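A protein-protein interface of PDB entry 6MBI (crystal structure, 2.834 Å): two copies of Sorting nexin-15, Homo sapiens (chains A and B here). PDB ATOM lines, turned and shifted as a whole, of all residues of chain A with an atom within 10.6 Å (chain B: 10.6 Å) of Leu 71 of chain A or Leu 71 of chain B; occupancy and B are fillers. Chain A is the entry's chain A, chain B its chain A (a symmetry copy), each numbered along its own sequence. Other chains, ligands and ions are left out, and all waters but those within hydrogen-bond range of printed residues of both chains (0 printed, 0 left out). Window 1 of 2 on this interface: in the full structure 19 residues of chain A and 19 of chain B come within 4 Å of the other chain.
Of chain B, only Leu 71 comes within 4 Å of Leu 71 of chain A.
Of chain A, only Leu 71 (3.9 Å) comes within 4 Å of Leu 71 of chain B.
No residue of chain A comes within 4 Å of Asn 70 of chain B.
Of the printed residues of chain B, His 68 of chain A touches Leu 75.
Of the printed residues of chain B, Phe 72 of chain A touches Arg 69 (3.5 Å).
Leu 115 of chain A touches none of the printed residues of chain B.
The nearest residue of chain A that does not touch Leu 71 of chain B is Phe 72 of chain A (4.5 Å).
The nearest printed residue of chain A that does not touch Phe 72 of chain B is Leu 71 of chain A (4.5 Å).
His 68 of chain A touches Leu 75 of chain B, and with the chains exchanged Leu 75 of chain A touches His 68 of chain B.
Arg 69 of chain A touches Phe 72 of chain B, and with the chains exchanged Phe 72 of chain A touches Arg 69 of chain B.
Arg 69 of chain A touches Leu 75 of chain B, and with the chains exchanged Leu 75 of chain A touches Arg 69 of chain B.
Leu 71 of chain B touches its own counterpart, Leu 71 of chain A.
16 positions are printed for both chains.
Of the 7 pairs that touch across the chains among the printed residues, 7 have their exchanged pair printed and touching as well.
Leu 75 of chain B touches His 68 of chain A.
Phe 72 of chain B touches Arg 69 of chain A (CE1 to CZ, 3.5 Å).
NH2 of Arg 69 of chain A touches C of Leu 75 of chain B, at 3.4 Å.
Leu 71 of chain A touches Leu 71 of chain B (CD1 to CB, 3.9 Å).
Phe 72 of chain A touches Arg 69 of chain B.
O of Leu 75 of chain A touches CE1 of His 68 of chain B, at 3.8 Å.
NH2 of Arg 69 of chain B touches C of Leu 75 of chain A (3.4 Å).
NE of Arg 69 of chain A lies within hydrogen-bond range of ND1 of His 68 of chain A (3.2 Å).
A ring nitrogen (ND1) of His 68 of chain B is in hydrogen-bond range of the guanidinium group (NE) of Arg 69 of chain B (3.2 Å).
Of the 16 printed residues of chain A, 5 touch a printed residue of chain B.
Hydrophobic or aromatic side chains of chain B within 4 Å of the printed part of chain A: His 68, Leu 71 and Phe 72.
Among the printed residues, 7 pairs touch across the chains.
Among the printed residues, no Asp or Glu carboxylate lies within 4 Å of a Lys or Arg side-chain nitrogen of the other chain.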
ATOM      1  N   LEU A  64       3.390 -26.816  -8.174  1.00  0.00           N
ATOM      2  CA  LEU A  64       3.264 -26.643  -9.618  1.00  0.00           C
ATOM      3  C   LEU A  64       2.423 -27.745 -10.253  1.00  0.00           C
ATOM      4  O   LEU A  64       1.621 -27.480 -11.145  1.00  0.00           O
ATOM      5  CB  LEU A  64       4.643 -26.604 -10.279  1.00  0.00           C
ATOM      6  CG  LEU A  64       5.513 -25.384  -9.979  1.00  0.00           C
ATOM      7  CD1 LEU A  64       6.878 -25.518 -10.638  1.00  0.00           C
ATOM      8  CD2 LEU A  64       4.814 -24.113 -10.433  1.00  0.00           C
ATOM      9  N   ALA A  65       2.617 -28.978  -9.796  1.00  0.00           N
ATOM     10  CA  ALA A  65       1.892 -30.123 -10.341  1.00  0.00           C
ATOM     11  C   ALA A  65       0.403 -30.021 -10.042  1.00  0.00           C
ATOM     12  O   ALA A  65      -0.426 -30.424 -10.860  1.00  0.00           O
ATOM     13  CB  ALA A  65       2.449 -31.425  -9.790  1.00  0.00           C
ATOM     14  N   TYR A  66       0.061 -29.492  -8.872  1.00  0.00           N
ATOM     15  CA  TYR A  66      -1.343 -29.239  -8.573  1.00  0.00           C
ATOM     16  C   TYR A  66      -1.834 -28.069  -9.412  1.00  0.00           C
ATOM     17  O   TYR A  66      -2.971 -28.072  -9.887  1.00  0.00           O
ATOM     18  CB  TYR A  66      -1.567 -28.954  -7.090  1.00  0.00           C
ATOM     19  CG  TYR A  66      -3.009 -28.630  -6.776  1.00  0.00           C
ATOM     20  CD1 TYR A  66      -3.966 -29.634  -6.709  1.00  0.00           C
ATOM     21  CD2 TYR A  66      -3.418 -27.319  -6.562  1.00  0.00           C
ATOM     22  CE1 TYR A  66      -5.288 -29.344  -6.431  1.00  0.00           C
ATOM     23  CE2 TYR A  66      -4.737 -27.020  -6.284  1.00  0.00           C
ATOM     24  CZ  TYR A  66      -5.667 -28.035  -6.218  1.00  0.00           C
ATOM     25  OH  TYR A  66      -6.982 -27.737  -5.940  1.00  0.00           O
ATOM     26  N   THR A  67      -0.969 -27.069  -9.587  1.00  0.00           N
ATOM     27  CA  THR A  67      -1.284 -25.929 -10.443  1.00  0.00           C
ATOM     28  C   THR A  67      -1.441 -26.410 -11.881  1.00  0.00           C
ATOM     29  O   THR A  67      -2.345 -25.982 -12.600  1.00  0.00           O
ATOM     30  CB  THR A  67      -0.196 -24.831 -10.376  1.00  0.00           C
ATOM     31  OG1 THR A  67      -0.016 -24.410  -9.019  1.00  0.00           O
ATOM     32  CG2 THR A  67      -0.589 -23.629 -11.225  1.00  0.00           C
ATOM     33  N   HIS A  68      -0.557 -27.316 -12.290  1.00  0.00           N
ATOM     34  CA  HIS A  68      -0.653 -27.950 -13.597  1.00  0.00           C
ATOM     35  C   HIS A  68      -1.792 -28.965 -13.579  1.00  0.00           C
ATOM     36  O   HIS A  68      -2.394 -29.210 -12.531  1.00  0.00           O
ATOM     37  CB  HIS A  68       0.672 -28.620 -13.971  1.00  0.00           C
ATOM     38  CG  HIS A  68       0.817 -28.910 -15.432  1.00  0.00           C
ATOM     39  ND1 HIS A  68       0.799 -30.190 -15.942  1.00  0.00           N
ATOM     40  CD2 HIS A  68       0.987 -28.085 -16.492  1.00  0.00           C
ATOM     41  CE1 HIS A  68       0.950 -30.141 -17.254  1.00  0.00           C
ATOM     42  NE2 HIS A  68       1.066 -28.875 -17.613  1.00  0.00           N
ATOM     43  N   ARG A  69      -2.088 -29.542 -14.741  1.00  0.00           N
ATOM     44  CA  ARG A  69      -3.179 -30.502 -14.897  1.00  0.00           C
ATOM     45  C   ARG A  69      -4.522 -29.900 -14.480  1.00  0.00           C
ATOM     46  O   ARG A  69      -5.429 -30.616 -14.054  1.00  0.00           O
ATOM     47  CB  ARG A  69      -2.902 -31.779 -14.095  1.00  0.00           C
ATOM     48  CG  ARG A  69      -1.532 -32.396 -14.343  1.00  0.00           C
ATOM     49  CD  ARG A  69      -1.328 -32.744 -15.809  1.00  0.00           C
ATOM     50  NE  ARG A  69       0.015 -33.256 -16.067  1.00  0.00           N
ATOM     51  CZ  ARG A  69       0.324 -34.547 -16.140  1.00  0.00           C
ATOM     52  NH1 ARG A  69      -0.618 -35.467 -15.981  1.00  0.00           N
ATOM     53  NH2 ARG A  69       1.575 -34.919 -16.377  1.00  0.00           N
ATOM     54  N   ASN A  70      -4.637 -28.580 -14.601  1.00  0.00           N
ATOM     55  CA  ASN A  70      -5.883 -27.877 -14.309  1.00  0.00           C
ATOM     56  C   ASN A  70      -6.557 -27.385 -15.582  1.00  0.00           C
ATOM     57  O   ASN A  70      -6.269 -26.288 -16.062  1.00  0.00           O
ATOM     58  CB  ASN A  70      -5.633 -26.696 -13.372  1.00  0.00           C
ATOM     59  CG  ASN A  70      -5.813 -27.059 -11.913  1.00  0.00           C
ATOM     60  OD1 ASN A  70      -5.018 -26.664 -11.062  1.00  0.00           O
ATOM     61  ND2 ASN A  70      -6.863 -27.814 -11.617  1.00  0.00           N
ATOM     62  N   LEU A  71      -7.454 -28.200 -16.127  1.00  0.00           N
ATOM     63  CA  LEU A  71      -8.115 -27.876 -17.387  1.00  0.00           C
ATOM     64  C   LEU A  71      -9.580 -28.309 -17.393  1.00  0.00           C
ATOM     65  O   LEU A  71     -10.016 -29.061 -16.519  1.00  0.00           O
ATOM     66  CB  LEU A  71      -7.378 -28.535 -18.557  1.00  0.00           C
ATOM     67  CG  LEU A  71      -5.925 -28.125 -18.814  1.00  0.00           C
ATOM     68  CD1 LEU A  71      -5.277 -29.051 -19.832  1.00  0.00           C
ATOM     69  CD2 LEU A  71      -5.847 -26.679 -19.277  1.00  0.00           C
ATOM     70  N   PHE A  72     -10.324 -27.810 -18.379  1.00  0.00           N
ATOM     71  CA  PHE A  72     -11.699 -28.231 -18.666  1.00  0.00           C
ATOM     72  C   PHE A  72     -12.705 -27.869 -17.571  1.00  0.00           C
ATOM     73  O   PHE A  72     -12.672 -28.421 -16.471  1.00  0.00           O
ATOM     74  CB  PHE A  72     -11.741 -29.741 -18.925  1.00  0.00           C
ATOM     75  CG  PHE A  72     -13.010 -30.212 -19.574  1.00  0.00           C
ATOM     76  CD1 PHE A  72     -13.165 -30.142 -20.948  1.00  0.00           C
ATOM     77  CD2 PHE A  72     -14.046 -30.730 -18.814  1.00  0.00           C
ATOM     78  CE1 PHE A  72     -14.329 -30.575 -21.552  1.00  0.00           C
ATOM     79  CE2 PHE A  72     -15.213 -31.165 -19.412  1.00  0.00           C
ATOM     80  CZ  PHE A  72     -15.354 -31.089 -20.784  1.00  0.00           C
ATOM     81  N   ARG A  73     -13.609 -26.946 -17.891  1.00  0.00           N
ATOM     82  CA  ARG A  73     -14.669 -26.544 -16.970  1.00  0.00           C
ATOM     83  C   ARG A  73     -15.951 -26.139 -17.698  1.00  0.00           C
ATOM     84  O   ARG A  73     -16.793 -25.438 -17.137  1.00  0.00           O
ATOM     85  CB  ARG A  73     -14.204 -25.388 -16.081  1.00  0.00           C
ATOM     86  CG  ARG A  73     -13.490 -25.818 -14.812  1.00  0.00           C
ATOM     87  CD  ARG A  73     -13.321 -24.649 -13.857  1.00  0.00           C
ATOM     88  NE  ARG A  73     -12.770 -25.069 -12.572  1.00  0.00           N
ATOM     89  CZ  ARG A  73     -13.502 -25.515 -11.556  1.00  0.00           C
ATOM     90  NH1 ARG A  73     -14.820 -25.602 -11.672  1.00  0.00           N
ATOM     91  NH2 ARG A  73     -12.915 -25.874 -10.422  1.00  0.00           N
ATOM     92  N   ARG A  74     -16.099 -26.581 -18.944  1.00  0.00           N
ATOM     93  CA  ARG A  74     -17.276 -26.234 -19.737  1.00  0.00           C
ATOM     94  C   ARG A  74     -17.635 -27.333 -20.735  1.00  0.00           C
ATOM     95  O   ARG A  74     -17.006 -28.390 -20.761  1.00  0.00           O
ATOM     96  CB  ARG A  74     -17.051 -24.915 -20.462  1.00  0.00           C
ATOM     97  N   LEU A  75     -18.650 -27.074 -21.555  1.00  0.00           N
ATOM     98  CA  LEU A  75     -19.113 -28.048 -22.539  1.00  0.00           C
ATOM     99  C   LEU A  75     -18.997 -27.507 -23.963  1.00  0.00           C
ATOM    100  O   LEU A  75     -18.007 -26.868 -24.315  1.00  0.00           O
ATOM    101  CB  LEU A  75     -20.562 -28.459 -22.257  1.00  0.00           C
ATOM    102  CG  LEU A  75     -20.855 -29.335 -21.034  1.00  0.00           C
ATOM    103  CD1 LEU A  75     -20.902 -28.510 -19.756  1.00  0.00           C
ATOM    104  CD2 LEU A  75     -22.166 -30.079 -21.228  1.00  0.00           C
ATOM    105  N   ILE A 112       4.780 -21.719 -20.107  1.00  0.00           N
ATOM    106  CA  ILE A 112       3.413 -21.789 -19.597  1.00  0.00           C
ATOM    107  C   ILE A 112       3.135 -20.607 -18.673  1.00  0.00           C
ATOM    108  O   ILE A 112       3.729 -20.504 -17.600  1.00  0.00           O
ATOM    109  CB  ILE A 112       3.145 -23.101 -18.834  1.00  0.00           C
ATOM    110  CG1 ILE A 112       3.408 -24.313 -19.732  1.00  0.00           C
ATOM    111  CG2 ILE A 112       1.716 -23.128 -18.308  1.00  0.00           C
ATOM    112  CD1 ILE A 112       3.164 -25.643 -19.053  1.00  0.00           C
ATOM    113  N   PRO A 113       2.230 -19.708 -19.095  1.00  0.00           N
ATOM    114  CA  PRO A 113       1.884 -18.490 -18.350  1.00  0.00           C
ATOM    115  C   PRO A 113       1.433 -18.768 -16.918  1.00  0.00           C
ATOM    116  O   PRO A 113       1.755 -17.996 -16.013  1.00  0.00           O
ATOM    117  CB  PRO A 113       0.736 -17.895 -19.171  1.00  0.00           C
ATOM    118  CG  PRO A 113       0.955 -18.413 -20.547  1.00  0.00           C
ATOM    119  CD  PRO A 113       1.496 -19.800 -20.368  1.00  0.00           C
ATOM    120  N   ALA A 114       0.699 -19.858 -16.721  1.00  0.00           N
ATOM    121  CA  ALA A 114       0.188 -20.209 -15.401  1.00  0.00           C
ATOM    122  C   ALA A 114       1.315 -20.596 -14.447  1.00  0.00           C
ATOM    123  O   ALA A 114       1.245 -20.329 -13.248  1.00  0.00           O
ATOM    124  CB  ALA A 114      -0.822 -21.340 -15.511  1.00  0.00           C
ATOM    125  N   LEU A 115       2.356 -21.224 -14.987  1.00  0.00           N
ATOM    126  CA  LEU A 115       3.484 -21.672 -14.179  1.00  0.00           C
ATOM    127  C   LEU A 115       4.573 -20.607 -14.092  1.00  0.00           C
ATOM    128  O   LEU A 115       5.246 -20.479 -13.070  1.00  0.00           O
ATOM    129  CB  LEU A 115       4.067 -22.968 -14.747  1.00  0.00           C
ATOM    130  CG  LEU A 115       3.110 -24.156 -14.851  1.00  0.00           C
ATOM    131  CD1 LEU A 115       3.839 -25.390 -15.362  1.00  0.00           C
ATOM    132  CD2 LEU A 115       2.451 -24.436 -13.509  1.00  0.00           C
ATOM    133  N   LEU B  64     -15.499 -26.269 -34.873  1.00  0.00           N
ATOM    134  CA  LEU B  64     -15.146 -25.703 -33.574  1.00  0.00           C
ATOM    135  C   LEU B  64     -14.975 -26.781 -32.510  1.00  0.00           C
ATOM    136  O   LEU B  64     -14.068 -26.704 -31.686  1.00  0.00           O
ATOM    137  CB  LEU B  64     -16.204 -24.696 -33.119  1.00  0.00           C
ATOM    138  CG  LEU B  64     -16.299 -23.395 -33.915  1.00  0.00           C
ATOM    139  CD1 LEU B  64     -17.439 -22.528 -33.401  1.00  0.00           C
ATOM    140  CD2 LEU B  64     -14.979 -22.644 -33.860  1.00  0.00           C
ATOM    141  N   ALA B  65     -15.854 -27.778 -32.528  1.00  0.00           N
ATOM    142  CA  ALA B  65     -15.812 -28.858 -31.546  1.00  0.00           C
ATOM    143  C   ALA B  65     -14.549 -29.691 -31.700  1.00  0.00           C
ATOM    144  O   ALA B  65     -13.989 -30.165 -30.710  1.00  0.00           O
ATOM    145  CB  ALA B  65     -17.042 -29.743 -31.664  1.00  0.00           C
ATOM    146  N   TYR B  66     -14.101 -29.879 -32.937  1.00  0.00           N
ATOM    147  CA  TYR B  66     -12.827 -30.550 -33.154  1.00  0.00           C
ATOM    148  C   TYR B  66     -11.693 -29.630 -32.726  1.00  0.00           C
ATOM    149  O   TYR B  66     -10.695 -30.084 -32.161  1.00  0.00           O
ATOM    150  CB  TYR B  66     -12.644 -30.969 -34.611  1.00  0.00           C
ATOM    151  CG  TYR B  66     -11.299 -31.612 -34.862  1.00  0.00           C
ATOM    152  CD1 TYR B  66     -11.054 -32.923 -34.473  1.00  0.00           C
ATOM    153  CD2 TYR B  66     -10.270 -30.905 -35.472  1.00  0.00           C
ATOM    154  CE1 TYR B  66      -9.824 -33.514 -34.691  1.00  0.00           C
ATOM    155  CE2 TYR B  66      -9.038 -31.489 -35.695  1.00  0.00           C
ATOM    156  CZ  TYR B  66      -8.821 -32.793 -35.304  1.00  0.00           C
ATOM    157  OH  TYR B  66      -7.594 -33.374 -35.527  1.00  0.00           O
ATOM    158  N   THR B  67     -11.852 -28.336 -33.003  1.00  0.00           N
ATOM    159  CA  THR B  67     -10.880 -27.336 -32.567  1.00  0.00           C
ATOM    160  C   THR B  67     -10.857 -27.290 -31.044  1.00  0.00           C
ATOM    161  O   THR B  67      -9.795 -27.202 -30.426  1.00  0.00           O
ATOM    162  CB  THR B  67     -11.198 -25.930 -33.127  1.00  0.00           C
ATOM    163  OG1 THR B  67     -11.266 -25.982 -34.558  1.00  0.00           O
ATOM    164  CG2 THR B  67     -10.130 -24.929 -32.714  1.00  0.00           C
ATOM    165  N   HIS B  68     -12.041 -27.361 -30.443  1.00  0.00           N
ATOM    166  CA  HIS B  68     -12.166 -27.444 -28.995  1.00  0.00           C
ATOM    167  C   HIS B  68     -11.769 -28.845 -28.537  1.00  0.00           C
ATOM    168  O   HIS B  68     -11.512 -29.722 -29.364  1.00  0.00           O
ATOM    169  CB  HIS B  68     -13.593 -27.109 -28.556  1.00  0.00           C
ATOM    170  CG  HIS B  68     -13.716 -26.744 -27.108  1.00  0.00           C
ATOM    171  ND1 HIS B  68     -14.340 -27.555 -26.187  1.00  0.00           N
ATOM    172  CD2 HIS B  68     -13.297 -25.652 -26.425  1.00  0.00           C
ATOM    173  CE1 HIS B  68     -14.300 -26.980 -24.998  1.00  0.00           C
ATOM    174  NE2 HIS B  68     -13.672 -25.824 -25.115  1.00  0.00           N
ATOM    175  N   ARG B  69     -11.710 -29.043 -27.223  1.00  0.00           N
ATOM    176  CA  ARG B  69     -11.306 -30.315 -26.628  1.00  0.00           C
ATOM    177  C   ARG B  69      -9.905 -30.727 -27.082  1.00  0.00           C
ATOM    178  O   ARG B  69      -9.582 -31.914 -27.132  1.00  0.00           O
ATOM    179  CB  ARG B  69     -12.315 -31.420 -26.960  1.00  0.00           C
ATOM    180  CG  ARG B  69     -13.765 -31.063 -26.661  1.00  0.00           C
ATOM    181  CD  ARG B  69     -13.966 -30.709 -25.195  1.00  0.00           C
ATOM    182  NE  ARG B  69     -15.336 -30.282 -24.922  1.00  0.00           N
ATOM    183  CZ  ARG B  69     -16.286 -31.077 -24.438  1.00  0.00           C
ATOM    184  NH1 ARG B  69     -16.016 -32.347 -24.165  1.00  0.00           N
ATOM    185  NH2 ARG B  69     -17.504 -30.601 -24.220  1.00  0.00           N
ATOM    186  N   ASN B  70      -9.080 -29.738 -27.415  1.00  0.00           N
ATOM    187  CA  ASN B  70      -7.692 -29.978 -27.798  1.00  0.00           C
ATOM    188  C   ASN B  70      -6.727 -29.524 -26.711  1.00  0.00           C
ATOM    189  O   ASN B  70      -6.321 -28.362 -26.677  1.00  0.00           O
ATOM    190  CB  ASN B  70      -7.359 -29.264 -29.108  1.00  0.00           C
ATOM    191  CG  ASN B  70      -7.562 -30.146 -30.323  1.00  0.00           C
ATOM    192  OD1 ASN B  70      -8.101 -29.708 -31.336  1.00  0.00           O
ATOM    193  ND2 ASN B  70      -7.128 -31.396 -30.224  1.00  0.00           N
ATOM    194  N   LEU B  71      -6.363 -30.444 -25.825  1.00  0.00           N
ATOM    195  CA  LEU B  71      -5.502 -30.117 -24.693  1.00  0.00           C
ATOM    196  C   LEU B  71      -4.515 -31.241 -24.380  1.00  0.00           C
ATOM    197  O   LEU B  71      -4.653 -32.356 -24.886  1.00  0.00           O
ATOM    198  CB  LEU B  71      -6.349 -29.815 -23.453  1.00  0.00           C
ATOM    199  CG  LEU B  71      -7.310 -28.624 -23.512  1.00  0.00           C
ATOM    200  CD1 LEU B  71      -8.244 -28.627 -22.311  1.00  0.00           C
ATOM    201  CD2 LEU B  71      -6.542 -27.314 -23.591  1.00  0.00           C
ATOM    202  N   PHE B  72      -3.519 -30.920 -23.557  1.00  0.00           N
ATOM    203  CA  PHE B  72      -2.571 -31.888 -22.996  1.00  0.00           C
ATOM    204  C   PHE B  72      -1.654 -32.537 -24.035  1.00  0.00           C
ATOM    205  O   PHE B  72      -2.098 -33.324 -24.870  1.00  0.00           O
ATOM    206  CB  PHE B  72      -3.328 -32.976 -22.225  1.00  0.00           C
ATOM    207  CG  PHE B  72      -2.456 -33.798 -21.321  1.00  0.00           C
ATOM    208  CD1 PHE B  72      -2.142 -33.352 -20.049  1.00  0.00           C
ATOM    209  CD2 PHE B  72      -1.955 -35.021 -21.739  1.00  0.00           C
ATOM    210  CE1 PHE B  72      -1.343 -34.104 -19.212  1.00  0.00           C
ATOM    211  CE2 PHE B  72      -1.154 -35.779 -20.906  1.00  0.00           C
ATOM    212  CZ  PHE B  72      -0.849 -35.320 -19.639  1.00  0.00           C
ATOM    213  N   ARG B  73      -0.365 -32.211 -23.960  1.00  0.00           N
ATOM    214  CA  ARG B  73       0.638 -32.798 -24.845  1.00  0.00           C
ATOM    215  C   ARG B  73       2.003 -32.930 -24.171  1.00  0.00           C
ATOM    216  O   ARG B  73       3.025 -33.045 -24.847  1.00  0.00           O
ATOM    217  CB  ARG B  73       0.782 -31.969 -26.124  1.00  0.00           C
ATOM    218  CG  ARG B  73      -0.182 -32.353 -27.233  1.00  0.00           C
ATOM    219  CD  ARG B  73       0.210 -31.698 -28.547  1.00  0.00           C
ATOM    220  NE  ARG B  73      -0.615 -32.168 -29.657  1.00  0.00           N
ATOM    221  CZ  ARG B  73      -0.355 -33.258 -30.371  1.00  0.00           C
ATOM    222  NH1 ARG B  73       0.709 -33.999 -30.092  1.00  0.00           N
ATOM    223  NH2 ARG B  73      -1.160 -33.610 -31.365  1.00  0.00           N
ATOM    224  N   ARG B  74       2.020 -32.915 -22.840  1.00  0.00           N
ATOM    225  CA  ARG B  74       3.274 -33.012 -22.097  1.00  0.00           C
ATOM    226  C   ARG B  74       3.083 -33.701 -20.746  1.00  0.00           C
ATOM    227  O   ARG B  74       1.989 -34.160 -20.422  1.00  0.00           O
ATOM    228  CB  ARG B  74       3.879 -31.630 -21.903  1.00  0.00           C
ATOM    229  N   LEU B  75       4.157 -33.769 -19.965  1.00  0.00           N
ATOM    230  CA  LEU B  75       4.120 -34.422 -18.660  1.00  0.00           C
ATOM    231  C   LEU B  75       4.469 -33.451 -17.533  1.00  0.00           C
ATOM    232  O   LEU B  75       4.028 -32.303 -17.533  1.00  0.00           O
ATOM    233  CB  LEU B  75       5.074 -35.621 -18.626  1.00  0.00           C
ATOM    234  CG  LEU B  75       4.713 -36.875 -19.429  1.00  0.00           C
ATOM    235  CD1 LEU B  75       5.063 -36.713 -20.902  1.00  0.00           C
ATOM    236  CD2 LEU B  75       5.423 -38.088 -18.849  1.00  0.00           C
ATOM    237  N   ILE B 112     -12.619 -17.469 -25.675  1.00  0.00           N
ATOM    238  CA  ILE B 112     -11.573 -18.442 -25.980  1.00  0.00           C
ATOM    239  C   ILE B 112     -10.799 -18.009 -27.222  1.00  0.00           C
ATOM    240  O   ILE B 112     -11.352 -17.981 -28.321  1.00  0.00           O
ATOM    241  CB  ILE B 112     -12.142 -19.856 -26.206  1.00  0.00           C
ATOM    242  CG1 ILE B 112     -12.923 -20.328 -24.977  1.00  0.00           C
ATOM    243  CG2 ILE B 112     -11.022 -20.834 -26.535  1.00  0.00           C
ATOM    244  CD1 ILE B 112     -13.513 -21.714 -25.121  1.00  0.00           C
ATOM    245  N   PRO B 113      -9.512 -17.665 -27.046  1.00  0.00           N
ATOM    246  CA  PRO B 113      -8.643 -17.180 -28.126  1.00  0.00           C
ATOM    247  C   PRO B 113      -8.570 -18.135 -29.315  1.00  0.00           C
ATOM    248  O   PRO B 113      -8.517 -17.684 -30.459  1.00  0.00           O
ATOM    249  CB  PRO B 113      -7.276 -17.063 -27.445  1.00  0.00           C
ATOM    250  CG  PRO B 113      -7.592 -16.861 -26.005  1.00  0.00           C
ATOM    251  CD  PRO B 113      -8.814 -17.692 -25.749  1.00  0.00           C
ATOM    252  N   ALA B 114      -8.571 -19.435 -29.041  1.00  0.00           N
ATOM    253  CA  ALA B 114      -8.476 -20.439 -30.093  1.00  0.00           C
ATOM    254  C   ALA B 114      -9.727 -20.456 -30.968  1.00  0.00           C
ATOM    255  O   ALA B 114      -9.652 -20.706 -32.171  1.00  0.00           O
ATOM    256  CB  ALA B 114      -8.236 -21.814 -29.491  1.00  0.00           C
ATOM    257  N   LEU B 115     -10.877 -20.185 -30.358  1.00  0.00           N
ATOM    258  CA  LEU B 115     -12.146 -20.196 -31.075  1.00  0.00           C
ATOM    259  C   LEU B 115     -12.486 -18.821 -31.644  1.00  0.00           C
ATOM    260  O   LEU B 115     -13.087 -18.713 -32.713  1.00  0.00           O
ATOM    261  CB  LEU B 115     -13.275 -20.674 -30.158  1.00  0.00           C
ATOM    262  CG  LEU B 115     -13.110 -22.065 -29.546  1.00  0.00           C
ATOM    263  CD1 LEU B 115     -14.332 -22.436 -28.719  1.00  0.00           C
ATOM    264  CD2 LEU B 115     -12.856 -23.103 -30.629  1.00  0.00           C
